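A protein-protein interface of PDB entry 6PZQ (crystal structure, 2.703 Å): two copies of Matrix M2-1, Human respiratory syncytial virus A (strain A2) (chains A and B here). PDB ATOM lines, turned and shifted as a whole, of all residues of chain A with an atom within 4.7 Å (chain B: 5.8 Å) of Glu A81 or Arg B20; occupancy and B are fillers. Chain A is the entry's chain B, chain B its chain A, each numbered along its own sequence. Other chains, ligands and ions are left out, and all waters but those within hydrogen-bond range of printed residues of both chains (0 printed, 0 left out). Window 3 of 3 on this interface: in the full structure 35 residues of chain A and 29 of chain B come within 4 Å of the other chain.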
ATOM      1  N   ALA A  73      31.600 -17.277   2.512  1.00  0.00           N
ATOM      2  CA  ALA A  73      31.988 -18.158   1.401  1.00  0.00           C
ATOM      3  C   ALA A  73      31.716 -17.532   0.039  1.00  0.00           C
ATOM      4  O   ALA A  73      32.410 -17.832  -0.939  1.00  0.00           O
ATOM      5  CB  ALA A  73      31.242 -19.491   1.497  1.00  0.00           C
ATOM      6  N   LEU A  74      30.680 -16.710  -0.028  1.00  0.00           N
ATOM      7  CA  LEU A  74      30.387 -15.882  -1.182  1.00  0.00           C
ATOM      8  C   LEU A  74      31.476 -14.852  -1.398  1.00  0.00           C
ATOM      9  O   LEU A  74      31.822 -14.521  -2.534  1.00  0.00           O
ATOM     10  CB  LEU A  74      29.053 -15.144  -0.968  1.00  0.00           C
ATOM     11  CG  LEU A  74      27.706 -15.842  -0.985  1.00  0.00           C
ATOM     12  CD1 LEU A  74      26.593 -14.898  -0.499  1.00  0.00           C
ATOM     13  CD2 LEU A  74      27.441 -16.286  -2.378  1.00  0.00           C
ATOM     14  N   VAL A  77      32.213 -10.275  -3.465  1.00  0.00           N
ATOM     15  CA  VAL A  77      31.744 -10.341  -4.824  1.00  0.00           C
ATOM     16  C   VAL A  77      30.527 -11.260  -4.910  1.00  0.00           C
ATOM     17  O   VAL A  77      29.557 -10.962  -5.590  1.00  0.00           O
ATOM     18  CB  VAL A  77      32.914 -10.793  -5.716  1.00  0.00           C
ATOM     19  CG1 VAL A  77      32.452 -11.093  -7.145  1.00  0.00           C
ATOM     20  CG2 VAL A  77      33.966  -9.760  -5.706  1.00  0.00           C
ATOM     21  N   GLY A  78      30.530 -12.347  -4.168  1.00  0.00           N
ATOM     22  CA  GLY A  78      29.378 -13.216  -4.165  1.00  0.00           C
ATOM     23  C   GLY A  78      28.164 -12.602  -3.503  1.00  0.00           C
ATOM     24  O   GLY A  78      27.038 -12.980  -3.822  1.00  0.00           O
ATOM     25  N   VAL A  79      28.365 -11.671  -2.570  1.00  0.00           N
ATOM     26  CA  VAL A  79      27.240 -11.017  -1.905  1.00  0.00           C
ATOM     27  C   VAL A  79      26.626  -9.992  -2.837  1.00  0.00           C
ATOM     28  O   VAL A  79      25.405  -9.772  -2.852  1.00  0.00           O
ATOM     29  CB  VAL A  79      27.717 -10.360  -0.593  1.00  0.00           C
ATOM     30  CG1 VAL A  79      26.781  -9.247  -0.142  1.00  0.00           C
ATOM     31  CG2 VAL A  79      27.900 -11.366   0.490  1.00  0.00           C
ATOM     32  N   LEU A  80      27.474  -9.322  -3.613  1.00  0.00           N
ATOM     33  CA  LEU A  80      26.973  -8.316  -4.536  1.00  0.00           C
ATOM     34  C   LEU A  80      26.223  -8.979  -5.686  1.00  0.00           C
ATOM     35  O   LEU A  80      25.149  -8.518  -6.076  1.00  0.00           O
ATOM     36  CB  LEU A  80      28.138  -7.464  -5.021  1.00  0.00           C
ATOM     37  CG  LEU A  80      28.802  -6.703  -3.873  1.00  0.00           C
ATOM     38  CD1 LEU A  80      30.140  -6.113  -4.329  1.00  0.00           C
ATOM     39  CD2 LEU A  80      27.903  -5.613  -3.367  1.00  0.00           C
ATOM     40  N   GLU A  81      26.733 -10.115  -6.171  1.00  0.00           N
ATOM     41  CA  GLU A  81      26.134 -10.799  -7.302  1.00  0.00           C
ATOM     42  C   GLU A  81      24.872 -11.537  -6.905  1.00  0.00           C
ATOM     43  O   GLU A  81      24.020 -11.813  -7.757  1.00  0.00           O
ATOM     44  CB  GLU A  81      27.115 -11.784  -7.901  1.00  0.00           C
ATOM     45  CG  GLU A  81      28.355 -11.132  -8.436  1.00  0.00           C
ATOM     46  CD  GLU A  81      29.418 -12.154  -8.850  1.00  0.00           C
ATOM     47  OE1 GLU A  81      29.561 -13.190  -8.167  1.00  0.00           O
ATOM     48  OE2 GLU A  81      30.090 -11.930  -9.877  1.00  0.00           O
ATOM     49  N   SER A  82      24.761 -11.917  -5.633  1.00  0.00           N
ATOM     50  CA  SER A  82      23.519 -12.518  -5.174  1.00  0.00           C
ATOM     51  C   SER A  82      22.471 -11.449  -4.972  1.00  0.00           C
ATOM     52  O   SER A  82      21.321 -11.624  -5.379  1.00  0.00           O
ATOM     53  CB  SER A  82      23.750 -13.294  -3.888  1.00  0.00           C
ATOM     54  OG  SER A  82      24.676 -14.357  -4.130  1.00  0.00           O
ATOM     55  N   TYR A  83      22.874 -10.310  -4.421  1.00  0.00           N
ATOM     56  CA  TYR A  83      21.960  -9.170  -4.353  1.00  0.00           C
ATOM     57  C   TYR A  83      21.445  -8.724  -5.725  1.00  0.00           C
ATOM     58  O   TYR A  83      20.253  -8.413  -5.839  1.00  0.00           O
ATOM     59  CB  TYR A  83      22.613  -7.995  -3.671  1.00  0.00           C
ATOM     60  CG  TYR A  83      21.689  -6.832  -3.560  1.00  0.00           C
ATOM     61  CD1 TYR A  83      20.783  -6.760  -2.517  1.00  0.00           C
ATOM     62  CD2 TYR A  83      21.723  -5.786  -4.480  1.00  0.00           C
ATOM     63  CE1 TYR A  83      19.925  -5.667  -2.374  1.00  0.00           C
ATOM     64  CE2 TYR A  83      20.851  -4.693  -4.350  1.00  0.00           C
ATOM     65  CZ  TYR A  83      19.959  -4.646  -3.287  1.00  0.00           C
ATOM     66  OH  TYR A  83      19.100  -3.589  -3.117  1.00  0.00           O
ATOM     67  N   ILE A  84      22.313  -8.631  -6.765  1.00  0.00           N
ATOM     68  CA  ILE A  84      21.825  -8.111  -8.046  1.00  0.00           C
ATOM     69  C   ILE A  84      20.732  -9.032  -8.550  1.00  0.00           C
ATOM     70  O   ILE A  84      19.691  -8.574  -9.029  1.00  0.00           O
ATOM     71  CB  ILE A  84      22.940  -7.929  -9.120  1.00  0.00           C
ATOM     72  CG1 ILE A  84      23.674  -9.243  -9.484  1.00  0.00           C
ATOM     73  CG2 ILE A  84      23.944  -6.803  -8.733  1.00  0.00           C
ATOM     74  CD1 ILE A  84      22.980 -10.216 -10.577  1.00  0.00           C
ATOM     75  N   GLY A  85      20.920 -10.350  -8.355  1.00  0.00           N
ATOM     76  CA  GLY A  85      20.038 -11.404  -8.787  1.00  0.00           C
ATOM     77  C   GLY A  85      18.973 -11.825  -7.788  1.00  0.00           C
ATOM     78  O   GLY A  85      18.220 -12.764  -8.082  1.00  0.00           O
ATOM     79  N   LEU A 165      31.322  -4.154 -10.520  1.00  0.00           N
ATOM     80  CA  LEU A 165      31.770  -5.551 -10.581  1.00  0.00           C
ATOM     81  C   LEU A 165      32.357  -5.913 -11.936  1.00  0.00           C
ATOM     82  O   LEU A 165      33.248  -6.764 -12.008  1.00  0.00           O
ATOM     83  CB  LEU A 165      30.618  -6.498 -10.259  1.00  0.00           C
ATOM     84  CG  LEU A 165      30.206  -6.738  -8.812  1.00  0.00           C
ATOM     85  CD1 LEU A 165      28.736  -6.865  -8.731  1.00  0.00           C
ATOM     86  CD2 LEU A 165      30.768  -8.008  -8.326  1.00  0.00           C
ATOM     87  N   ASN B  17      36.489 -12.747  -3.569  1.00  0.00           N
ATOM     88  CA  ASN B  17      35.639 -13.861  -3.981  1.00  0.00           C
ATOM     89  C   ASN B  17      35.271 -14.795  -2.825  1.00  0.00           C
ATOM     90  O   ASN B  17      34.095 -15.020  -2.564  1.00  0.00           O
ATOM     91  CB  ASN B  17      36.334 -14.632  -5.080  1.00  0.00           C
ATOM     92  CG  ASN B  17      36.038 -14.066  -6.422  1.00  0.00           C
ATOM     93  OD1 ASN B  17      36.894 -13.445  -7.099  1.00  0.00           O
ATOM     94  ND2 ASN B  17      34.789 -14.262  -6.828  1.00  0.00           N
ATOM     95  N   GLY B  18      36.245 -15.326  -2.108  1.00  0.00           N
ATOM     96  CA  GLY B  18      36.014 -16.214  -0.977  1.00  0.00           C
ATOM     97  C   GLY B  18      36.381 -17.639  -1.320  1.00  0.00           C
ATOM     98  O   GLY B  18      37.163 -17.915  -2.249  1.00  0.00           O
ATOM     99  N   LYS B  19      35.761 -18.579  -0.577  1.00  0.00           N
ATOM    100  CA  LYS B  19      36.048 -19.980  -0.853  1.00  0.00           C
ATOM    101  C   LYS B  19      35.732 -20.383  -2.300  1.00  0.00           C
ATOM    102  O   LYS B  19      36.071 -21.510  -2.676  1.00  0.00           O
ATOM    103  CB  LYS B  19      35.304 -20.893   0.119  1.00  0.00           C
ATOM    104  CG  LYS B  19      33.780 -21.123  -0.199  1.00  0.00           C
ATOM    105  CD  LYS B  19      33.401 -22.492  -0.936  1.00  0.00           C
ATOM    106  CE  LYS B  19      31.858 -22.730  -0.965  1.00  0.00           C
ATOM    107  NZ  LYS B  19      31.373 -23.753  -2.022  1.00  0.00           N
ATOM    108  N   ARG B  20      35.100 -19.512  -3.115  1.00  0.00           N
ATOM    109  CA  ARG B  20      34.910 -19.798  -4.550  1.00  0.00           C
ATOM    110  C   ARG B  20      36.191 -19.701  -5.374  1.00  0.00           C
ATOM    111  O   ARG B  20      36.258 -20.320  -6.438  1.00  0.00           O
ATOM    112  CB  ARG B  20      33.889 -18.851  -5.208  1.00  0.00           C
ATOM    113  CG  ARG B  20      32.561 -18.719  -4.471  1.00  0.00           C
ATOM    114  CD  ARG B  20      31.987 -17.294  -4.534  1.00  0.00           C
ATOM    115  NE  ARG B  20      31.040 -17.178  -5.627  1.00  0.00           N
ATOM    116  CZ  ARG B  20      30.833 -16.081  -6.319  1.00  0.00           C
ATOM    117  NH1 ARG B  20      31.523 -14.994  -6.032  1.00  0.00           N
ATOM    118  NH2 ARG B  20      29.938 -16.092  -7.304  1.00  0.00           N
ATOM    119  N   CYS B  21      37.195 -18.928  -4.941  1.00  0.00           N
ATOM    120  CA  CYS B  21      38.396 -18.731  -5.745  1.00  0.00           C
ATOM    121  C   CYS B  21      39.342 -19.875  -5.423  1.00  0.00           C
ATOM    122  O   CYS B  21      39.718 -20.072  -4.263  1.00  0.00           O
ATOM    123  CB  CYS B  21      39.054 -17.367  -5.501  1.00  0.00           C
ATOM    124  SG  CYS B  21      40.731 -17.148  -6.407  1.00  0.00           S
ATOM    125  N   HIS B  22      39.692 -20.638  -6.449  1.00  0.00           N
ATOM    126  CA  HIS B  22      40.545 -21.812  -6.340  1.00  0.00           C
ATOM    127  C   HIS B  22      41.981 -21.510  -6.747  1.00  0.00           C
ATOM    128  O   HIS B  22      42.682 -22.358  -7.323  1.00  0.00           O
ATOM    129  CB  HIS B  22      39.946 -22.923  -7.188  1.00  0.00           C
ATOM    130  CG  HIS B  22      38.537 -23.214  -6.808  1.00  0.00           C
ATOM    131  ND1 HIS B  22      37.517 -23.304  -7.731  1.00  0.00           N
ATOM    132  CD2 HIS B  22      37.967 -23.376  -5.587  1.00  0.00           C
ATOM    133  CE1 HIS B  22      36.383 -23.541  -7.094  1.00  0.00           C
ATOM    134  NE2 HIS B  22      36.630 -23.595  -5.794  1.00  0.00           N
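N of Gly A78 lies close to NH1 of Arg B20, at 3.4 Å. The guanidinium group (NH2) of Arg B20 lies within salt-bridge range of the side-chain carboxylate (OE1) of Glu A81 (3.1 Å). The backbone NH of Lys B19 is in hydrogen-bond range of the backbone carbonyl oxygen of Ala A73 (3.5 Å). The backbone carbonyl oxygen (O) of Leu A74 lies close to the backbone carbonyl oxygen (O) of Asn B17, at 2.3 Å.
O of Arg B20 lies close to NE2 of His B22, at 3.4 Å. NH1 of Arg B20 sits close to ND2 of Asn B17 (3.4 Å). The backbone carbonyl oxygen (O) of Gly A78 lies within hydrogen-bond range of the side-chain hydroxyl (OG) of Ser A82.
O of Asn B17 touches O of Ala A73 (3.7 Å). Ala A73 touches Gly B18 (O to CA, 3.95 Å). Ala A73 touches Arg B20. Leu A74 touches Arg B20. Val A77 touches Asn B17 (CG1 to ND2, 3.95 Å).
Of the printed residues of chain B, Leu A74 touches Asn B17 and Arg B20. Of the printed residues of chain B, Val A77 touches Asn B17. Glu A81 touches just one residue of chain B: Arg B20. Tyr A83 touches none of the printed residues of chain B. Of the printed residues of chain A, Asn B17 touches Ala A73, Leu A74 and Val A77. Of the printed residues of chain A, Gly B18 touches Ala A73 (3.95 Å). Arg B20 touches four residues of chain A. The nearest residue of chain A that does not touch Arg B20 is Val A77 (4.02 Å).
Of the 6 printed residues of chain B, 4 touch a printed residue of chain A. Of the 12 printed residues of chain A, 5 touch a printed residue of chain B. Among the printed residues, Asp or Glu carboxylates within 4 Å of a Lys or Arg side-chain nitrogen of the other chain: Glu A81 with Arg B20.
No position is printed for both chains.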
